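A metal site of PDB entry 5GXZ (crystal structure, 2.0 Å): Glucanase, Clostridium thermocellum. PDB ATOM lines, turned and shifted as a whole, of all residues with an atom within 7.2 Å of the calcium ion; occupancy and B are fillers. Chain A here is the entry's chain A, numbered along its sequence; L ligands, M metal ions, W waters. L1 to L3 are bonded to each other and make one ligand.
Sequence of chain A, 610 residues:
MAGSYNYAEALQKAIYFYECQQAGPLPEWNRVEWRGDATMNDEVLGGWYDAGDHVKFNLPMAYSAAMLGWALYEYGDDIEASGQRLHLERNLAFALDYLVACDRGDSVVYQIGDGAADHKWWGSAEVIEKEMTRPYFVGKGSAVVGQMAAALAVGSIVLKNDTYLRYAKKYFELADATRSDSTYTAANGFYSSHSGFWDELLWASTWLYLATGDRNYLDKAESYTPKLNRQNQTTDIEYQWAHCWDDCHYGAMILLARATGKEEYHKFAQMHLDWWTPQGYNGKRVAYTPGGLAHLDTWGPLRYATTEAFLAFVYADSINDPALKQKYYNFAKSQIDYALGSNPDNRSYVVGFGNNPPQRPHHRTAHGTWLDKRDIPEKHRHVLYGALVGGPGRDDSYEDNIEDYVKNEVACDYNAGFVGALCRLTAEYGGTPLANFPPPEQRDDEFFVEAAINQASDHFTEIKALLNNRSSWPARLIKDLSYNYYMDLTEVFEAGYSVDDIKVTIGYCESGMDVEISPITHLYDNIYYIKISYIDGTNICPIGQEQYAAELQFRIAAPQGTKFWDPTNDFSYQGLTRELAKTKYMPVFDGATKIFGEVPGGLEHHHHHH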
ATOM      1  N   LEU A  59     -12.737 -22.466 -10.464  1.00  0.00           N
ATOM      2  CA  LEU A  59     -13.654 -22.902  -9.424  1.00  0.00           C
ATOM      3  C   LEU A  59     -15.043 -23.246  -9.964  1.00  0.00           C
ATOM      4  O   LEU A  59     -15.465 -24.385  -9.770  1.00  0.00           O
ATOM      5  CB  LEU A  59     -13.647 -21.979  -8.198  1.00  0.00           C
ATOM      6  CG  LEU A  59     -14.482 -22.303  -6.949  1.00  0.00           C
ATOM      7  CD1 LEU A  59     -14.170 -23.650  -6.330  1.00  0.00           C
ATOM      8  CD2 LEU A  59     -14.287 -21.225  -5.895  1.00  0.00           C
ATOM      9  N   ALA A 143      -9.658 -24.418  -2.058  1.00  0.00           N
ATOM     10  CA  ALA A 143     -11.002 -24.494  -2.637  1.00  0.00           C
ATOM     11  C   ALA A 143     -10.944 -24.837  -4.121  1.00  0.00           C
ATOM     12  O   ALA A 143     -11.573 -25.802  -4.553  1.00  0.00           O
ATOM     13  CB  ALA A 143     -11.791 -23.209  -2.403  1.00  0.00           C
ATOM     14  N   GLN A 147     -11.888 -28.458  -5.611  1.00  0.00           N
ATOM     15  CA  GLN A 147     -12.950 -28.621  -6.588  1.00  0.00           C
ATOM     16  C   GLN A 147     -12.479 -29.306  -7.859  1.00  0.00           C
ATOM     17  O   GLN A 147     -13.186 -30.163  -8.421  1.00  0.00           O
ATOM     18  CB  GLN A 147     -13.591 -27.284  -6.961  1.00  0.00           C
ATOM     19  CG  GLN A 147     -14.867 -27.477  -7.759  1.00  0.00           C
ATOM     20  CD  GLN A 147     -15.939 -28.212  -6.977  1.00  0.00           C
ATOM     21  OE1 GLN A 147     -16.365 -29.303  -7.366  1.00  0.00           O
ATOM     22  NE2 GLN A 147     -16.372 -27.633  -5.868  1.00  0.00           N
ATOM     23  N   ASP A 181      -6.517 -20.733   1.212  1.00  0.00           N
ATOM     24  CA  ASP A 181      -6.959 -20.060  -0.009  1.00  0.00           C
ATOM     25  C   ASP A 181      -6.129 -18.819  -0.353  1.00  0.00           C
ATOM     26  O   ASP A 181      -6.501 -18.027  -1.242  1.00  0.00           O
ATOM     27  CB  ASP A 181      -8.439 -19.658   0.078  1.00  0.00           C
ATOM     28  CG  ASP A 181      -9.375 -20.817  -0.171  1.00  0.00           C
ATOM     29  OD1 ASP A 181      -9.016 -21.746  -0.927  1.00  0.00           O
ATOM     30  OD2 ASP A 181     -10.484 -20.798   0.414  1.00  0.00           O
ATOM     31  N   SER A 193     -13.454 -17.004  -2.738  1.00  0.00           N
ATOM     32  CA  SER A 193     -13.774 -18.095  -1.826  1.00  0.00           C
ATOM     33  C   SER A 193     -14.418 -17.531  -0.563  1.00  0.00           C
ATOM     34  O   SER A 193     -13.721 -17.035   0.319  1.00  0.00           O
ATOM     35  CB  SER A 193     -12.567 -18.961  -1.490  1.00  0.00           C
ATOM     36  OG  SER A 193     -12.928 -19.992  -0.591  1.00  0.00           O
ATOM     37  N   HIS A 194     -15.746 -17.551  -0.509  1.00  0.00           N
ATOM     38  CA  HIS A 194     -16.526 -17.000   0.595  1.00  0.00           C
ATOM     39  C   HIS A 194     -16.646 -17.999   1.744  1.00  0.00           C
ATOM     40  O   HIS A 194     -16.550 -17.608   2.903  1.00  0.00           O
ATOM     41  CB  HIS A 194     -17.965 -16.678   0.143  1.00  0.00           C
ATOM     42  CG  HIS A 194     -18.038 -15.744  -1.020  1.00  0.00           C
ATOM     43  ND1 HIS A 194     -18.184 -14.388  -0.879  1.00  0.00           N
ATOM     44  CD2 HIS A 194     -18.018 -15.980  -2.357  1.00  0.00           C
ATOM     45  CE1 HIS A 194     -18.234 -13.822  -2.067  1.00  0.00           C
ATOM     46  NE2 HIS A 194     -18.132 -14.759  -2.984  1.00  0.00           N
ATOM     47  N   SER A 195     -16.879 -19.263   1.431  1.00  0.00           N
ATOM     48  CA  SER A 195     -17.188 -20.227   2.470  1.00  0.00           C
ATOM     49  C   SER A 195     -15.927 -20.775   3.132  1.00  0.00           C
ATOM     50  O   SER A 195     -16.007 -21.402   4.197  1.00  0.00           O
ATOM     51  CB  SER A 195     -18.059 -21.350   1.901  1.00  0.00           C
ATOM     52  OG  SER A 195     -17.364 -22.064   0.888  1.00  0.00           O
ATOM     53  N   GLY A 196     -14.767 -20.537   2.514  1.00  0.00           N
ATOM     54  CA  GLY A 196     -13.538 -21.220   2.901  1.00  0.00           C
ATOM     55  C   GLY A 196     -13.372 -22.526   2.143  1.00  0.00           C
ATOM     56  O   GLY A 196     -14.131 -22.810   1.218  1.00  0.00           O
ATOM     57  N   PHE A 197     -12.412 -23.344   2.548  1.00  0.00           N
ATOM     58  CA  PHE A 197     -12.029 -24.490   1.730  1.00  0.00           C
ATOM     59  C   PHE A 197     -12.395 -25.841   2.329  1.00  0.00           C
ATOM     60  O   PHE A 197     -12.248 -26.874   1.658  1.00  0.00           O
ATOM     61  CB  PHE A 197     -10.531 -24.472   1.430  1.00  0.00           C
ATOM     62  CG  PHE A 197      -9.675 -24.509   2.662  1.00  0.00           C
ATOM     63  CD1 PHE A 197      -9.503 -25.692   3.373  1.00  0.00           C
ATOM     64  CD2 PHE A 197      -9.087 -23.352   3.135  1.00  0.00           C
ATOM     65  CE1 PHE A 197      -8.735 -25.722   4.521  1.00  0.00           C
ATOM     66  CE2 PHE A 197      -8.317 -23.365   4.301  1.00  0.00           C
ATOM     67  CZ  PHE A 197      -8.146 -24.563   4.980  1.00  0.00           C
ATOM     68  N   TRP A 198     -12.872 -25.847   3.567  1.00  0.00           N
ATOM     69  CA  TRP A 198     -13.201 -27.103   4.231  1.00  0.00           C
ATOM     70  C   TRP A 198     -14.258 -27.885   3.467  1.00  0.00           C
ATOM     71  O   TRP A 198     -14.145 -29.100   3.357  1.00  0.00           O
ATOM     72  CB  TRP A 198     -13.556 -26.907   5.713  1.00  0.00           C
ATOM     73  CG  TRP A 198     -12.389 -26.394   6.528  1.00  0.00           C
ATOM     74  CD1 TRP A 198     -12.267 -25.157   7.094  1.00  0.00           C
ATOM     75  CD2 TRP A 198     -11.199 -27.118   6.883  1.00  0.00           C
ATOM     76  NE1 TRP A 198     -11.084 -25.063   7.779  1.00  0.00           N
ATOM     77  CE2 TRP A 198     -10.401 -26.243   7.658  1.00  0.00           C
ATOM     78  CE3 TRP A 198     -10.713 -28.396   6.604  1.00  0.00           C
ATOM     79  CZ2 TRP A 198      -9.149 -26.612   8.152  1.00  0.00           C
ATOM     80  CZ3 TRP A 198      -9.469 -28.765   7.104  1.00  0.00           C
ATOM     81  CH2 TRP A 198      -8.697 -27.875   7.866  1.00  0.00           C
ATOM     82  N   ASP A 199     -15.230 -27.182   2.873  1.00  0.00           N
ATOM     83  CA  ASP A 199     -16.259 -27.871   2.085  1.00  0.00           C
ATOM     84  C   ASP A 199     -15.727 -28.575   0.823  1.00  0.00           C
ATOM     85  O   ASP A 199     -16.134 -29.699   0.530  1.00  0.00           O
ATOM     86  CB  ASP A 199     -17.430 -26.941   1.765  1.00  0.00           C
ATOM     87  CG  ASP A 199     -17.012 -25.712   0.973  1.00  0.00           C
ATOM     88  OD1 ASP A 199     -16.587 -24.704   1.570  1.00  0.00           O
ATOM     89  OD2 ASP A 199     -17.115 -25.766  -0.267  1.00  0.00           O
ATOM     90  N   GLU A 200     -14.815 -27.945   0.094  1.00  0.00           N
ATOM     91  CA  GLU A 200     -14.171 -28.564  -1.049  1.00  0.00           C
ATOM     92  C   GLU A 200     -13.375 -29.810  -0.661  1.00  0.00           C
ATOM     93  O   GLU A 200     -13.396 -30.799  -1.402  1.00  0.00           O
ATOM     94  CB  GLU A 200     -13.259 -27.579  -1.804  1.00  0.00           C
ATOM     95  CG  GLU A 200     -14.005 -26.494  -2.588  1.00  0.00           C
ATOM     96  CD  GLU A 200     -14.486 -25.351  -1.699  1.00  0.00           C
ATOM     97  OE1 GLU A 200     -14.110 -25.302  -0.496  1.00  0.00           O
ATOM     98  OE2 GLU A 200     -15.232 -24.477  -2.205  1.00  0.00           O
ATOM     99  N   LEU A 201     -12.669 -29.787   0.463  1.00  0.00           N
ATOM    100  CA  LEU A 201     -11.932 -30.966   0.910  1.00  0.00           C
ATOM    101  C   LEU A 201     -12.925 -32.099   1.225  1.00  0.00           C
ATOM    102  O   LEU A 201     -12.697 -33.255   0.855  1.00  0.00           O
ATOM    103  CB  LEU A 201     -11.020 -30.654   2.107  1.00  0.00           C
ATOM    104  CG  LEU A 201      -9.816 -29.713   1.902  1.00  0.00           C
ATOM    105  CD1 LEU A 201      -9.029 -29.541   3.205  1.00  0.00           C
ATOM    106  CD2 LEU A 201      -8.876 -30.190   0.788  1.00  0.00           C
ATOM    107  N   ASN A 229     -18.613 -24.354   8.292  1.00  0.00           N
ATOM    108  CA  ASN A 229     -19.271 -23.207   8.914  1.00  0.00           C
ATOM    109  C   ASN A 229     -20.578 -23.604   9.598  1.00  0.00           C
ATOM    110  O   ASN A 229     -21.265 -24.530   9.162  1.00  0.00           O
ATOM    111  CB  ASN A 229     -19.528 -22.093   7.887  1.00  0.00           C
ATOM    112  CG  ASN A 229     -18.256 -21.710   7.147  1.00  0.00           C
ATOM    113  OD1 ASN A 229     -18.273 -21.492   5.931  1.00  0.00           O
ATOM    114  ND2 ASN A 229     -17.149 -21.634   7.866  1.00  0.00           N
ATOM    115  N   CYS A 244     -23.508 -25.010  -4.543  1.00  0.00           N
ATOM    116  CA  CYS A 244     -23.155 -24.028  -5.546  1.00  0.00           C
ATOM    117  C   CYS A 244     -21.649 -24.035  -5.778  1.00  0.00           C
ATOM    118  O   CYS A 244     -20.916 -24.713  -5.062  1.00  0.00           O
ATOM    119  CB  CYS A 244     -23.616 -22.624  -5.140  1.00  0.00           C
ATOM    120  SG  CYS A 244     -22.812 -22.039  -3.654  1.00  0.00           S
ATOM    121  N   TRP A 245     -21.199 -23.275  -6.759  1.00  0.00           N
ATOM    122  CA  TRP A 245     -19.767 -23.232  -7.089  1.00  0.00           C
ATOM    123  C   TRP A 245     -18.837 -22.994  -5.891  1.00  0.00           C
ATOM    124  O   TRP A 245     -17.684 -23.418  -5.929  1.00  0.00           O
ATOM    125  CB  TRP A 245     -19.511 -22.209  -8.186  1.00  0.00           C
ATOM    126  CG  TRP A 245     -19.911 -20.825  -7.771  1.00  0.00           C
ATOM    127  CD1 TRP A 245     -21.108 -20.215  -8.018  1.00  0.00           C
ATOM    128  CD2 TRP A 245     -19.123 -19.880  -7.034  1.00  0.00           C
ATOM    129  NE1 TRP A 245     -21.108 -18.945  -7.485  1.00  0.00           N
ATOM    130  CE2 TRP A 245     -19.904 -18.718  -6.859  1.00  0.00           C
ATOM    131  CE3 TRP A 245     -17.827 -19.903  -6.499  1.00  0.00           C
ATOM    132  CZ2 TRP A 245     -19.428 -17.573  -6.210  1.00  0.00           C
ATOM    133  CZ3 TRP A 245     -17.348 -18.784  -5.818  1.00  0.00           C
ATOM    134  CH2 TRP A 245     -18.150 -17.633  -5.684  1.00  0.00           C
ATOM    135  N   ASP A 246     -19.324 -22.314  -4.839  1.00  0.00           N
ATOM    136  CA  ASP A 246     -18.504 -21.908  -3.697  1.00  0.00           C
ATOM    137  C   ASP A 246     -18.508 -22.886  -2.520  1.00  0.00           C
ATOM    138  O   ASP A 246     -17.623 -22.854  -1.647  1.00  0.00           O
ATOM    139  CB  ASP A 246     -18.959 -20.524  -3.193  1.00  0.00           C
ATOM    140  CG  ASP A 246     -18.053 -19.985  -2.098  1.00  0.00           C
ATOM    141  OD1 ASP A 246     -16.907 -19.628  -2.434  1.00  0.00           O
ATOM    142  OD2 ASP A 246     -18.473 -19.906  -0.910  1.00  0.00           O
ATOM    143  N   ASP A 247     -19.516 -23.772  -2.498  1.00  0.00           N
ATOM    144  CA  ASP A 247     -19.877 -24.524  -1.307  1.00  0.00           C
ATOM    145  C   ASP A 247     -20.706 -25.765  -1.621  1.00  0.00           C
ATOM    146  O   ASP A 247     -21.920 -25.704  -1.889  1.00  0.00           O
ATOM    147  CB  ASP A 247     -20.604 -23.629  -0.305  1.00  0.00           C
ATOM    148  CG  ASP A 247     -20.789 -24.274   1.065  1.00  0.00           C
ATOM    149  OD1 ASP A 247     -20.491 -25.479   1.247  1.00  0.00           O
ATOM    150  OD2 ASP A 247     -21.240 -23.540   1.979  1.00  0.00           O
ATOM    151  N   CYS A 248     -19.995 -26.879  -1.582  1.00  0.00           N
ATOM    152  CA  CYS A 248     -20.522 -28.186  -1.963  1.00  0.00           C
ATOM    153  C   CYS A 248     -20.741 -29.092  -0.754  1.00  0.00           C
ATOM    154  O   CYS A 248     -20.916 -30.301  -0.922  1.00  0.00           O
ATOM    155  CB  CYS A 248     -19.550 -28.848  -2.944  1.00  0.00           C
ATOM    156  SG  CYS A 248     -19.738 -28.176  -4.621  1.00  0.00           S
ATOM    157  N   HIS A 249     -20.726 -28.538   0.459  1.00  0.00           N
ATOM    158  CA  HIS A 249     -20.936 -29.405   1.618  1.00  0.00           C
ATOM    159  C   HIS A 249     -22.330 -30.037   1.636  1.00  0.00           C
ATOM    160  O   HIS A 249     -22.466 -31.177   2.070  1.00  0.00           O
ATOM    161  CB  HIS A 249     -20.532 -28.735   2.936  1.00  0.00           C
ATOM    162  CG  HIS A 249     -21.557 -27.824   3.534  1.00  0.00           C
ATOM    163  ND1 HIS A 249     -21.629 -26.478   3.223  1.00  0.00           N
ATOM    164  CD2 HIS A 249     -22.496 -28.034   4.486  1.00  0.00           C
ATOM    165  CE1 HIS A 249     -22.599 -25.914   3.925  1.00  0.00           C
ATOM    166  NE2 HIS A 249     -23.138 -26.837   4.700  1.00  0.00           N
HETATM  167  C1  LIG L   1     -22.489 -15.194  -9.122  1.00  0.00           C
HETATM  168  C2  LIG L   1     -23.005 -15.195  -7.683  1.00  0.00           C
HETATM  169  C3  LIG L   1     -22.061 -14.404  -6.790  1.00  0.00           C
HETATM  170  C4  LIG L   1     -21.721 -13.019  -7.340  1.00  0.00           C
HETATM  171  C5  LIG L   1     -20.519 -12.437  -6.589  1.00  0.00           C
HETATM  172  C6  LIG L   1     -22.304 -13.763  -9.604  1.00  0.00           C
HETATM  173  O1  LIG L   1     -21.751 -13.752 -10.908  1.00  0.00           O
HETATM  174  O2  LIG L   1     -23.440 -15.853  -9.955  1.00  0.00           O
HETATM  175  O3  LIG L   1     -23.136 -16.542  -7.195  1.00  0.00           O
HETATM  176  O4  LIG L   1     -22.658 -14.222  -5.496  1.00  0.00           O
HETATM  177  O5  LIG L   1     -21.390 -13.096  -8.737  1.00  0.00           O
HETATM  178  O6  LIG L   1     -19.451 -13.406  -6.572  1.00  0.00           O
HETATM  179  C1  LG2 L   2     -22.489 -14.216  -3.248  1.00  0.00           C
HETATM  180  C2  LG2 L   2     -21.829 -14.935  -2.083  1.00  0.00           C
HETATM  181  C3  LG2 L   2     -22.130 -16.416  -2.198  1.00  0.00           C
HETATM  182  C4  LG2 L   2     -21.674 -16.979  -3.555  1.00  0.00           C
HETATM  183  C5  LG2 L   2     -22.069 -18.436  -3.730  1.00  0.00           C
HETATM  184  C6  LG2 L   2     -21.908 -14.867  -4.497  1.00  0.00           C
HETATM  185  O1  LG2 L   2     -22.156 -12.835  -3.165  1.00  0.00           O
HETATM  186  O2  LG2 L   2     -22.401 -14.442  -0.865  1.00  0.00           O
HETATM  187  O3  LG2 L   2     -21.515 -17.065  -1.095  1.00  0.00           O
HETATM  188  O4  LG2 L   2     -22.346 -16.228  -4.563  1.00  0.00           O
HETATM  189  O5  LG2 L   2     -23.475 -18.574  -3.453  1.00  0.00           O
HETATM  190  C1  LG3 L   3     -21.416 -18.913   0.609  1.00  0.00           C
HETATM  191  C2  LG3 L   3     -22.309 -19.524   1.682  1.00  0.00           C
HETATM  192  C3  LG3 L   3     -22.833 -18.423   2.610  1.00  0.00           C
HETATM  193  C4  LG3 L   3     -23.592 -17.407   1.762  1.00  0.00           C
HETATM  194  C5  LG3 L   3     -24.168 -16.298   2.629  1.00  0.00           C
HETATM  195  C6  LG3 L   3     -22.235 -17.885  -0.156  1.00  0.00           C
HETATM  196  O1  LG3 L   3     -20.922 -19.980  -0.214  1.00  0.00           O
HETATM  197  O2  LG3 L   3     -21.509 -20.440   2.416  1.00  0.00           O
HETATM  198  O3  LG3 L   3     -23.667 -18.996   3.617  1.00  0.00           O
HETATM  199  O4  LG3 L   3     -22.716 -16.890   0.755  1.00  0.00           O
HETATM  200  O5  LG3 L   3     -23.230 -15.238   2.859  1.00  0.00           O
HETATM  201 CA    CA M   1     -15.856 -23.422  -0.233  1.00  0.00          CA
HETATM  202  O   HOH W   1     -15.057 -21.496  -1.046  1.00  0.00           O
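The side-chain carboxylate of Asp 246 lies within hydrogen-bond range of an oxygen (O1) of LG3 L3 (2.5 Å). The side-chain carboxylate of Asp 247 lies within hydrogen-bond range of an oxygen (O2) of LG3 L3. NE1 of Trp 245 is in hydrogen-bond range of O3 of LIG L1 (3.2 Å). The side-chain sulfur (SG) of Cys 244 lies within hydrogen-bond range of an oxygen (O5) of LG2 L2 (3.5 Å).
OD1 of Asn 229 lies close to O of Ser 195, 2.9 Å away. The backbone NH (N) of Cys 248 sits close to the side-chain carboxylate (OD2) of Asp 199. The side-chain carboxylate (OD1) of Asp 246 is in hydrogen-bond range of the backbone NH (N) of His 194. The side-chain sulfur (SG) of Cys 244 lies close to the backbone NH (N) of Asp 246, at 3.7 Å.
Within 4 Å of the calcium ion: Ser 195, Gly 196, Asp 199, Glu 200 and Asp 246.
The calcium ion is bound by water W1, at 2.2 Å. The side-chain hydroxyl (OG) of Ser 195 is bound to the calcium ion (2.3 Å). The calcium ion is bound by OE2 of Glu 200, 2.3 Å away. The calcium ion is bound by OD1 of Asp 199 (2.3 Å). The calcium ion is bound by O of Asp 246 (2.3 Å). O of Gly 196 binds the calcium ion (2.3 Å). The side-chain carboxylate (OE1) of Glu 200 binds the calcium ion (2.6 Å). OD2 of Asp 199 binds the calcium ion (2.7 Å). The calcium ion has eight donor atoms within binding distance.
Water W1 lies within hydrogen-bond range of OG of Ser 193 (2.6 Å) and OD1 of Asp 246 (3.0 Å).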
